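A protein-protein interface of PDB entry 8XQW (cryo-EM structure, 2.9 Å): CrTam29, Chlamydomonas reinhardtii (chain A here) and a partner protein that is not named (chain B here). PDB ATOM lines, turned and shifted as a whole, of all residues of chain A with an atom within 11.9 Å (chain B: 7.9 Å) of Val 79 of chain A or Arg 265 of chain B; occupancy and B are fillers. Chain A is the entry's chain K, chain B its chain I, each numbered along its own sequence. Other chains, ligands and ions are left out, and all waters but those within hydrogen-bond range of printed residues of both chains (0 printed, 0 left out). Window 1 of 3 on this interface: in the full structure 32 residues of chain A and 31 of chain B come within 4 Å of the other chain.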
ATOM      1  N   THR A  67      10.459  19.608 -27.870  1.00  0.00           N
ATOM      2  CA  THR A  67      10.360  20.575 -26.784  1.00  0.00           C
ATOM      3  C   THR A  67       9.672  19.995 -25.558  1.00  0.00           C
ATOM      4  O   THR A  67       8.733  19.207 -25.671  1.00  0.00           O
ATOM      5  CB  THR A  67       9.595  21.835 -27.217  1.00  0.00           C
ATOM      6  OG1 THR A  67       9.167  22.555 -26.056  1.00  0.00           O
ATOM      7  CG2 THR A  67       8.385  21.462 -28.054  1.00  0.00           C
ATOM      8  N   SER A  68      10.163  20.381 -24.382  1.00  0.00           N
ATOM      9  CA  SER A  68       9.484  20.019 -23.143  1.00  0.00           C
ATOM     10  C   SER A  68       8.494  21.098 -22.728  1.00  0.00           C
ATOM     11  O   SER A  68       7.460  20.801 -22.123  1.00  0.00           O
ATOM     12  CB  SER A  68      10.507  19.778 -22.032  1.00  0.00           C
ATOM     13  OG  SER A  68      10.902  21.000 -21.434  1.00  0.00           O
ATOM     14  N   ALA A  69       8.787  22.348 -23.076  1.00  0.00           N
ATOM     15  CA  ALA A  69       8.091  23.522 -22.573  1.00  0.00           C
ATOM     16  C   ALA A  69       6.586  23.438 -22.820  1.00  0.00           C
ATOM     17  O   ALA A  69       6.151  23.492 -23.979  1.00  0.00           O
ATOM     18  CB  ALA A  69       8.663  24.766 -23.236  1.00  0.00           C
ATOM     19  N   ILE A  72       5.788  28.091 -22.767  1.00  0.00           N
ATOM     20  CA  ILE A  72       6.531  29.100 -23.509  1.00  0.00           C
ATOM     21  C   ILE A  72       7.849  28.502 -23.960  1.00  0.00           C
ATOM     22  O   ILE A  72       8.578  27.911 -23.157  1.00  0.00           O
ATOM     23  CB  ILE A  72       6.772  30.352 -22.652  1.00  0.00           C
ATOM     24  CG1 ILE A  72       5.591  30.623 -21.728  1.00  0.00           C
ATOM     25  CG2 ILE A  72       6.960  31.548 -23.532  1.00  0.00           C
ATOM     26  CD1 ILE A  72       4.353  31.053 -22.447  1.00  0.00           C
ATOM     27  N   SER A  73       8.172  28.673 -25.238  1.00  0.00           N
ATOM     28  CA  SER A  73       9.379  28.090 -25.815  1.00  0.00           C
ATOM     29  C   SER A  73       9.907  28.995 -26.913  1.00  0.00           C
ATOM     30  O   SER A  73       9.369  29.023 -28.027  1.00  0.00           O
ATOM     31  CB  SER A  73       9.103  26.690 -26.358  1.00  0.00           C
ATOM     32  OG  SER A  73       8.428  26.765 -27.598  1.00  0.00           O
ATOM     33  N   PRO A  74      10.964  29.752 -26.636  1.00  0.00           N
ATOM     34  CA  PRO A  74      11.646  30.488 -27.707  1.00  0.00           C
ATOM     35  C   PRO A  74      12.299  29.543 -28.702  1.00  0.00           C
ATOM     36  O   PRO A  74      12.284  28.325 -28.507  1.00  0.00           O
ATOM     37  CB  PRO A  74      12.681  31.323 -26.950  1.00  0.00           C
ATOM     38  CG  PRO A  74      12.135  31.431 -25.577  1.00  0.00           C
ATOM     39  CD  PRO A  74      11.479  30.123 -25.311  1.00  0.00           C
ATOM     40  N   MET A  75      12.881  30.081 -29.771  1.00  0.00           N
ATOM     41  CA  MET A  75      13.432  29.208 -30.797  1.00  0.00           C
ATOM     42  C   MET A  75      14.774  28.605 -30.417  1.00  0.00           C
ATOM     43  O   MET A  75      15.248  27.709 -31.120  1.00  0.00           O
ATOM     44  CB  MET A  75      13.548  29.955 -32.123  1.00  0.00           C
ATOM     45  CG  MET A  75      12.201  30.236 -32.761  1.00  0.00           C
ATOM     46  SD  MET A  75      11.551  28.791 -33.624  1.00  0.00           S
ATOM     47  CE  MET A  75      11.307  29.445 -35.271  1.00  0.00           C
ATOM     48  N   THR A  76      15.403  29.070 -29.343  1.00  0.00           N
ATOM     49  CA  THR A  76      16.600  28.408 -28.870  1.00  0.00           C
ATOM     50  C   THR A  76      16.377  27.871 -27.463  1.00  0.00           C
ATOM     51  O   THR A  76      15.987  28.626 -26.568  1.00  0.00           O
ATOM     52  CB  THR A  76      17.812  29.350 -28.876  1.00  0.00           C
ATOM     53  OG1 THR A  76      18.837  28.814 -28.033  1.00  0.00           O
ATOM     54  CG2 THR A  76      17.431  30.732 -28.400  1.00  0.00           C
ATOM     55  N   PRO A  77      16.606  26.581 -27.239  1.00  0.00           N
ATOM     56  CA  PRO A  77      16.250  25.987 -25.948  1.00  0.00           C
ATOM     57  C   PRO A  77      17.000  26.638 -24.802  1.00  0.00           C
ATOM     58  O   PRO A  77      18.134  27.090 -24.948  1.00  0.00           O
ATOM     59  CB  PRO A  77      16.645  24.516 -26.116  1.00  0.00           C
ATOM     60  CG  PRO A  77      17.631  24.511 -27.221  1.00  0.00           C
ATOM     61  CD  PRO A  77      17.222  25.604 -28.145  1.00  0.00           C
ATOM     62  N   TYR A  78      16.338  26.695 -23.655  1.00  0.00           N
ATOM     63  CA  TYR A  78      16.885  27.361 -22.484  1.00  0.00           C
ATOM     64  C   TYR A  78      17.825  26.410 -21.764  1.00  0.00           C
ATOM     65  O   TYR A  78      17.425  25.308 -21.382  1.00  0.00           O
ATOM     66  CB  TYR A  78      15.753  27.805 -21.568  1.00  0.00           C
ATOM     67  CG  TYR A  78      16.142  28.029 -20.134  1.00  0.00           C
ATOM     68  CD1 TYR A  78      16.737  29.207 -19.734  1.00  0.00           C
ATOM     69  CD2 TYR A  78      15.888  27.072 -19.176  1.00  0.00           C
ATOM     70  CE1 TYR A  78      17.077  29.420 -18.423  1.00  0.00           C
ATOM     71  CE2 TYR A  78      16.230  27.278 -17.867  1.00  0.00           C
ATOM     72  CZ  TYR A  78      16.823  28.451 -17.497  1.00  0.00           C
ATOM     73  OH  TYR A  78      17.169  28.658 -16.191  1.00  0.00           O
ATOM     74  N   VAL A  79      19.067  26.829 -21.588  1.00  0.00           N
ATOM     75  CA  VAL A  79      20.076  26.044 -20.886  1.00  0.00           C
ATOM     76  C   VAL A  79      20.206  26.592 -19.471  1.00  0.00           C
ATOM     77  O   VAL A  79      20.527  27.773 -19.310  1.00  0.00           O
ATOM     78  CB  VAL A  79      21.427  26.076 -21.624  1.00  0.00           C
ATOM     79  CG1 VAL A  79      21.793  27.495 -22.030  1.00  0.00           C
ATOM     80  CG2 VAL A  79      22.509  25.478 -20.760  1.00  0.00           C
ATOM     81  N   PRO A  80      19.960  25.792 -18.440  1.00  0.00           N
ATOM     82  CA  PRO A  80      19.910  26.345 -17.084  1.00  0.00           C
ATOM     83  C   PRO A  80      21.290  26.743 -16.596  1.00  0.00           C
ATOM     84  O   PRO A  80      22.085  25.897 -16.190  1.00  0.00           O
ATOM     85  CB  PRO A  80      19.342  25.189 -16.253  1.00  0.00           C
ATOM     86  CG  PRO A  80      18.739  24.248 -17.239  1.00  0.00           C
ATOM     87  CD  PRO A  80      19.554  24.382 -18.474  1.00  0.00           C
ATOM     88  N   GLU A  81      21.567  28.041 -16.606  1.00  0.00           N
ATOM     89  CA  GLU A  81      22.850  28.528 -16.118  1.00  0.00           C
ATOM     90  C   GLU A  81      22.846  28.517 -14.601  1.00  0.00           C
ATOM     91  O   GLU A  81      21.819  28.774 -13.969  1.00  0.00           O
ATOM     92  CB  GLU A  81      23.164  29.939 -16.624  1.00  0.00           C
ATOM     93  CG  GLU A  81      22.060  30.956 -16.429  1.00  0.00           C
ATOM     94  CD  GLU A  81      21.035  30.925 -17.545  1.00  0.00           C
ATOM     95  OE1 GLU A  81      20.050  31.690 -17.479  1.00  0.00           O
ATOM     96  OE2 GLU A  81      21.228  30.153 -18.500  1.00  0.00           O
ATOM     97  N   GLU A  82      24.000  28.219 -14.017  1.00  0.00           N
ATOM     98  CA  GLU A  82      24.108  28.068 -12.578  1.00  0.00           C
ATOM     99  C   GLU A  82      25.014  29.144 -11.999  1.00  0.00           C
ATOM    100  O   GLU A  82      25.571  29.974 -12.722  1.00  0.00           O
ATOM    101  CB  GLU A  82      24.629  26.678 -12.214  1.00  0.00           C
ATOM    102  CG  GLU A  82      23.788  25.995 -11.164  1.00  0.00           C
ATOM    103  CD  GLU A  82      22.427  25.593 -11.698  1.00  0.00           C
ATOM    104  OE1 GLU A  82      21.533  25.273 -10.888  1.00  0.00           O
ATOM    105  OE2 GLU A  82      22.249  25.590 -12.932  1.00  0.00           O
ATOM    106  N   GLU A  83      25.132  29.134 -10.678  1.00  0.00           N
ATOM    107  CA  GLU A  83      26.019  30.065 -10.006  1.00  0.00           C
ATOM    108  C   GLU A  83      27.436  29.927 -10.553  1.00  0.00           C
ATOM    109  O   GLU A  83      27.860  28.824 -10.910  1.00  0.00           O
ATOM    110  CB  GLU A  83      26.013  29.803  -8.498  1.00  0.00           C
ATOM    111  CG  GLU A  83      26.560  28.430  -8.097  1.00  0.00           C
ATOM    112  CD  GLU A  83      27.376  28.456  -6.804  1.00  0.00           C
ATOM    113  OE1 GLU A  83      28.161  29.405  -6.599  1.00  0.00           O
ATOM    114  OE2 GLU A  83      27.236  27.515  -5.995  1.00  0.00           O
ATOM    115  N   LYS A 244      35.356  26.581 -22.781  1.00  0.00           N
ATOM    116  CA  LYS A 244      34.665  27.163 -21.644  1.00  0.00           C
ATOM    117  C   LYS A 244      35.475  26.963 -20.370  1.00  0.00           C
ATOM    118  O   LYS A 244      36.218  25.986 -20.249  1.00  0.00           O
ATOM    119  CB  LYS A 244      33.286  26.529 -21.470  1.00  0.00           C
ATOM    120  CG  LYS A 244      32.466  26.511 -22.730  1.00  0.00           C
ATOM    121  CD  LYS A 244      31.189  25.715 -22.540  1.00  0.00           C
ATOM    122  CE  LYS A 244      29.976  26.620 -22.545  1.00  0.00           C
ATOM    123  NZ  LYS A 244      30.065  27.643 -21.475  1.00  0.00           N
ATOM    124  N   PRO A 247      34.900  24.517 -14.117  1.00  0.00           N
ATOM    125  CA  PRO A 247      34.293  24.820 -12.822  1.00  0.00           C
ATOM    126  C   PRO A 247      35.051  24.154 -11.683  1.00  0.00           C
ATOM    127  O   PRO A 247      35.748  23.160 -11.856  1.00  0.00           O
ATOM    128  CB  PRO A 247      32.879  24.249 -12.951  1.00  0.00           C
ATOM    129  CG  PRO A 247      32.703  23.951 -14.381  1.00  0.00           C
ATOM    130  CD  PRO A 247      34.049  23.622 -14.900  1.00  0.00           C
ATOM    131  N   GLU B 140      11.113  24.597 -17.352  1.00  0.00           N
ATOM    132  CA  GLU B 140      12.226  24.950 -16.494  1.00  0.00           C
ATOM    133  C   GLU B 140      12.456  26.438 -16.355  1.00  0.00           C
ATOM    134  O   GLU B 140      12.994  26.862 -15.333  1.00  0.00           O
ATOM    135  CB  GLU B 140      13.516  24.339 -17.015  1.00  0.00           C
ATOM    136  CG  GLU B 140      13.427  22.882 -17.324  1.00  0.00           C
ATOM    137  CD  GLU B 140      14.715  22.360 -17.903  1.00  0.00           C
ATOM    138  OE1 GLU B 140      15.518  21.787 -17.137  1.00  0.00           O
ATOM    139  OE2 GLU B 140      14.932  22.533 -19.121  1.00  0.00           O
ATOM    140  N   GLU B 141      12.092  27.244 -17.343  1.00  0.00           N
ATOM    141  CA  GLU B 141      12.699  28.559 -17.356  1.00  0.00           C
ATOM    142  C   GLU B 141      12.058  29.506 -16.364  1.00  0.00           C
ATOM    143  O   GLU B 141      12.572  29.699 -15.264  1.00  0.00           O
ATOM    144  CB  GLU B 141      12.581  29.147 -18.750  1.00  0.00           C
ATOM    145  CG  GLU B 141      13.433  30.347 -18.980  1.00  0.00           C
ATOM    146  CD  GLU B 141      13.611  30.627 -20.441  1.00  0.00           C
ATOM    147  OE1 GLU B 141      12.871  30.035 -21.248  1.00  0.00           O
ATOM    148  OE2 GLU B 141      14.489  31.436 -20.790  1.00  0.00           O
ATOM    149  N   ARG B 149      12.677  36.750 -23.132  1.00  0.00           N
ATOM    150  CA  ARG B 149      13.697  36.225 -24.025  1.00  0.00           C
ATOM    151  C   ARG B 149      13.164  36.057 -25.434  1.00  0.00           C
ATOM    152  O   ARG B 149      13.840  36.406 -26.405  1.00  0.00           O
ATOM    153  CB  ARG B 149      14.198  34.893 -23.497  1.00  0.00           C
ATOM    154  CG  ARG B 149      15.504  34.473 -24.068  1.00  0.00           C
ATOM    155  CD  ARG B 149      16.142  33.454 -23.173  1.00  0.00           C
ATOM    156  NE  ARG B 149      15.352  32.239 -23.137  1.00  0.00           N
ATOM    157  CZ  ARG B 149      15.441  31.276 -24.040  1.00  0.00           C
ATOM    158  NH1 ARG B 149      16.293  31.383 -25.041  1.00  0.00           N
ATOM    159  NH2 ARG B 149      14.681  30.203 -23.935  1.00  0.00           N
ATOM    160  N   ASP B 210      26.997  20.561 -27.813  1.00  0.00           N
ATOM    161  CA  ASP B 210      26.263  20.218 -26.603  1.00  0.00           C
ATOM    162  C   ASP B 210      25.170  19.226 -26.958  1.00  0.00           C
ATOM    163  O   ASP B 210      24.077  19.607 -27.371  1.00  0.00           O
ATOM    164  CB  ASP B 210      25.692  21.467 -25.950  1.00  0.00           C
ATOM    165  CG  ASP B 210      25.766  21.408 -24.450  1.00  0.00           C
ATOM    166  OD1 ASP B 210      26.803  21.818 -23.894  1.00  0.00           O
ATOM    167  OD2 ASP B 210      24.797  20.938 -23.823  1.00  0.00           O
ATOM    168  N   TRP B 211      25.468  17.943 -26.798  1.00  0.00           N
ATOM    169  CA  TRP B 211      24.519  16.889 -27.110  1.00  0.00           C
ATOM    170  C   TRP B 211      23.635  16.519 -25.936  1.00  0.00           C
ATOM    171  O   TRP B 211      22.666  15.783 -26.126  1.00  0.00           O
ATOM    172  CB  TRP B 211      25.249  15.637 -27.577  1.00  0.00           C
ATOM    173  CG  TRP B 211      25.967  15.805 -28.845  1.00  0.00           C
ATOM    174  CD1 TRP B 211      27.309  15.808 -29.023  1.00  0.00           C
ATOM    175  CD2 TRP B 211      25.388  15.976 -30.131  1.00  0.00           C
ATOM    176  NE1 TRP B 211      27.608  15.981 -30.343  1.00  0.00           N
ATOM    177  CE2 TRP B 211      26.440  16.083 -31.048  1.00  0.00           C
ATOM    178  CE3 TRP B 211      24.078  16.048 -30.599  1.00  0.00           C
ATOM    179  CZ2 TRP B 211      26.225  16.260 -32.403  1.00  0.00           C
ATOM    180  CZ3 TRP B 211      23.869  16.226 -31.940  1.00  0.00           C
ATOM    181  CH2 TRP B 211      24.935  16.329 -32.829  1.00  0.00           C
ATOM    182  N   GLY B 212      23.954  16.983 -24.736  1.00  0.00           N
ATOM    183  CA  GLY B 212      23.106  16.777 -23.583  1.00  0.00           C
ATOM    184  C   GLY B 212      23.634  15.819 -22.545  1.00  0.00           C
ATOM    185  O   GLY B 212      22.959  15.613 -21.533  1.00  0.00           O
ATOM    186  N   ASP B 213      24.806  15.228 -22.738  1.00  0.00           N
ATOM    187  CA  ASP B 213      25.367  14.301 -21.771  1.00  0.00           C
ATOM    188  C   ASP B 213      26.678  14.837 -21.217  1.00  0.00           C
ATOM    189  O   ASP B 213      27.057  15.980 -21.452  1.00  0.00           O
ATOM    190  CB  ASP B 213      25.590  12.935 -22.403  1.00  0.00           C
ATOM    191  CG  ASP B 213      26.263  13.033 -23.721  1.00  0.00           C
ATOM    192  OD1 ASP B 213      26.547  14.167 -24.138  1.00  0.00           O
ATOM    193  OD2 ASP B 213      26.518  11.985 -24.342  1.00  0.00           O
ATOM    194  N   HIS B 214      27.342  14.012 -20.464  1.00  0.00           N
ATOM    195  CA  HIS B 214      28.643  14.378 -19.938  1.00  0.00           C
ATOM    196  C   HIS B 214      29.720  13.988 -20.943  1.00  0.00           C
ATOM    197  O   HIS B 214      29.596  12.966 -21.612  1.00  0.00           O
ATOM    198  CB  HIS B 214      28.889  13.682 -18.604  1.00  0.00           C
ATOM    199  CG  HIS B 214      29.955  14.313 -17.769  1.00  0.00           C
ATOM    200  ND1 HIS B 214      31.230  13.804 -17.682  1.00  0.00           N
ATOM    201  CD2 HIS B 214      29.935  15.405 -16.977  1.00  0.00           C
ATOM    202  CE1 HIS B 214      31.951  14.558 -16.877  1.00  0.00           C
ATOM    203  NE2 HIS B 214      31.189  15.538 -16.437  1.00  0.00           N
ATOM    204  N   ALA B 260      23.739   6.957 -15.541  1.00  0.00           N
ATOM    205  CA  ALA B 260      23.238   8.209 -14.989  1.00  0.00           C
ATOM    206  C   ALA B 260      23.852   9.418 -15.668  1.00  0.00           C
ATOM    207  O   ALA B 260      23.230  10.478 -15.708  1.00  0.00           O
ATOM    208  CB  ALA B 260      23.499   8.277 -13.491  1.00  0.00           C
ATOM    209  N   MET B 261      25.049   9.292 -16.199  1.00  0.00           N
ATOM    210  CA  MET B 261      25.714  10.429 -16.832  1.00  0.00           C
ATOM    211  C   MET B 261      25.205  10.729 -18.170  1.00  0.00           C
ATOM    212  O   MET B 261      25.875  11.457 -18.867  1.00  0.00           O
ATOM    213  CB  MET B 261      27.214  10.175 -16.923  1.00  0.00           C
ATOM    214  CG  MET B 261      28.016  10.919 -15.910  1.00  0.00           C
ATOM    215  SD  MET B 261      29.787  10.808 -16.171  1.00  0.00           S
ATOM    216  CE  MET B 261      29.983   9.058 -16.310  1.00  0.00           C
ATOM    217  N   SER B 262      24.072  10.216 -18.614  1.00  0.00           N
ATOM    218  CA  SER B 262      23.582  10.498 -19.951  1.00  0.00           C
ATOM    219  C   SER B 262      22.619  11.660 -19.986  1.00  0.00           C
ATOM    220  O   SER B 262      22.014  11.908 -21.026  1.00  0.00           O
ATOM    221  CB  SER B 262      22.907   9.273 -20.534  1.00  0.00           C
ATOM    222  OG  SER B 262      21.922   8.800 -19.658  1.00  0.00           O
ATOM    223  N   ASP B 263      22.446  12.366 -18.876  1.00  0.00           N
ATOM    224  CA  ASP B 263      21.711  13.623 -18.837  1.00  0.00           C
ATOM    225  C   ASP B 263      22.320  14.453 -17.717  1.00  0.00           C
ATOM    226  O   ASP B 263      21.995  14.251 -16.548  1.00  0.00           O
ATOM    227  CB  ASP B 263      20.231  13.395 -18.618  1.00  0.00           C
ATOM    228  CG  ASP B 263      19.400  14.565 -19.078  1.00  0.00           C
ATOM    229  OD1 ASP B 263      19.753  15.713 -18.742  1.00  0.00           O
ATOM    230  OD2 ASP B 263      18.399  14.339 -19.785  1.00  0.00           O
ATOM    231  N   ALA B 264      23.182  15.400 -18.079  1.00  0.00           N
ATOM    232  CA  ALA B 264      24.046  16.036 -17.098  1.00  0.00           C
ATOM    233  C   ALA B 264      23.388  17.201 -16.379  1.00  0.00           C
ATOM    234  O   ALA B 264      23.980  17.752 -15.447  1.00  0.00           O
ATOM    235  CB  ALA B 264      25.321  16.519 -17.774  1.00  0.00           C
ATOM    236  N   ARG B 265      22.187  17.600 -16.782  1.00  0.00           N
ATOM    237  CA  ARG B 265      21.562  18.754 -16.151  1.00  0.00           C
ATOM    238  C   ARG B 265      20.827  18.364 -14.878  1.00  0.00           C
ATOM    239  O   ARG B 265      20.649  19.194 -13.982  1.00  0.00           O
ATOM    240  CB  ARG B 265      20.613  19.425 -17.133  1.00  0.00           C
ATOM    241  CG  ARG B 265      21.266  19.800 -18.440  1.00  0.00           C
ATOM    242  CD  ARG B 265      22.545  20.567 -18.189  1.00  0.00           C
ATOM    243  NE  ARG B 265      22.768  21.603 -19.189  1.00  0.00           N
ATOM    244  CZ  ARG B 265      23.389  21.404 -20.345  1.00  0.00           C
ATOM    245  NH1 ARG B 265      23.549  22.407 -21.193  1.00  0.00           N
ATOM    246  NH2 ARG B 265      23.850  20.204 -20.655  1.00  0.00           N
ATOM    247  N   CYS B 266      20.400  17.111 -14.774  1.00  0.00           N
ATOM    248  CA  CYS B 266      19.589  16.671 -13.653  1.00  0.00           C
ATOM    249  C   CYS B 266      20.428  16.606 -12.388  1.00  0.00           C
ATOM    250  O   CYS B 266      21.598  16.980 -12.365  1.00  0.00           O
ATOM    251  CB  CYS B 266      18.988  15.309 -13.948  1.00  0.00           C
ATOM    252  SG  CYS B 266      18.756  15.028 -15.686  1.00  0.00           S
ATOM    253  N   VAL B 267      19.816  16.132 -11.312  1.00  0.00           N
ATOM    254  CA  VAL B 267      20.542  15.832 -10.085  1.00  0.00           C
ATOM    255  C   VAL B 267      21.206  14.462 -10.208  1.00  0.00           C
ATOM    256  O   VAL B 267      22.395  14.326  -9.867  1.00  0.00           O
ATOM    257  CB  VAL B 267      19.615  15.927  -8.868  1.00  0.00           C
ATOM    258  CG1 VAL B 267      20.400  15.848  -7.595  1.00  0.00           C
ATOM    259  CG2 VAL B 267      18.851  17.208  -8.930  1.00  0.00           C
ATOM    260  N   PRO B 268      20.511  13.420 -10.680  1.00  0.00           N
ATOM    261  CA  PRO B 268      21.221  12.168 -10.960  1.00  0.00           C
ATOM    262  C   PRO B 268      22.378  12.334 -11.921  1.00  0.00           C
ATOM    263  O   PRO B 268      23.363  11.595 -11.818  1.00  0.00           O
ATOM    264  CB  PRO B 268      20.125  11.269 -11.545  1.00  0.00           C
ATOM    265  CG  PRO B 268      18.985  12.136 -11.798  1.00  0.00           C
ATOM    266  CD  PRO B 268      19.063  13.221 -10.819  1.00  0.00           C
ATOM    267  N   GLY B 269      22.312  13.298 -12.832  1.00  0.00           N
ATOM    268  CA  GLY B 269      23.428  13.516 -13.731  1.00  0.00           C
ATOM    269  C   GLY B 269      24.695  13.930 -13.012  1.00  0.00           C
ATOM    270  O   GLY B 269      25.795  13.765 -13.534  1.00  0.00           O
ATOM    271  N   ALA B 270      24.558  14.482 -11.809  1.00  0.00           N
ATOM    272  CA  ALA B 270      25.724  14.885 -11.032  1.00  0.00           C
ATOM    273  C   ALA B 270      26.141  13.800 -10.054  1.00  0.00           C
ATOM    274  O   ALA B 270      27.342  13.564  -9.843  1.00  0.00           O
ATOM    275  CB  ALA B 270      25.432  16.180 -10.285  1.00  0.00           C
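The backbone carbonyl oxygen (O) of Thr 76 of chain A lies within hydrogen-bond range of the guanidinium group (NH1) of Arg 149 of chain B.
The guanidinium group (NH1) of Arg 265 of chain B is in salt-bridge range of the side-chain carboxylate (OD2) of Asp 210 of chain B (3.3 Å). The backbone carbonyl oxygen (O) of Val 79 of chain A lies close to the side-chain carboxylate (OE2) of Glu 81 of chain A, 2.6 Å away. The side-chain carboxylate of Glu 141 of chain B is in salt-bridge range of the guanidinium group of Arg 149 of chain B (2.6 Å).
Among the printed residues, merely in contact across the chains: Pro 74 of chain A with Arg 149 of chain B (3.3 Å), Tyr 78 of chain A with Glu 141 of chain B (3.3 Å), Tyr 78 of chain A with Arg 149 of chain B (3.5 Å) and Val 79 of chain A with Arg 265 of chain B (3.3 Å).
Printed residues of chain B within 4 Å of Thr 76 of chain A: Arg 149. Printed residues of chain A within 4 Å of Arg 149 of chain B: Pro 74, Thr 76 and Tyr 78. No residue of chain A comes within 4 Å of Asp 210 of chain B. Ala 264 of chain B touches none of the printed residues of chain A. Of chain A, only Val 79 (3.3 Å) comes within 4 Å of Arg 265 of chain B. No residue of chain A comes within 4 Å of Cys 266 of chain B. Val 267 of chain B touches none of the printed residues of chain A. No residue of chain A comes within 4 Å of Gly 269 of chain B. The nearest residue of chain B that does not touch Val 79 of chain A is Asp 210 of chain B (5.9 Å). The nearest residue of chain A that does not touch Arg 265 of chain B is Pro 80 of chain A (4.3 Å).
Printed residues of chain A that touch a printed residue of chain B: Pro 74, Thr 76, Tyr 78 and Val 79. Of the 19 printed residues of chain B, 3 touch a printed residue of chain A. Printed residues of chain B that touch a printed residue of chain A: Glu 141, Arg 149 and Arg 265.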
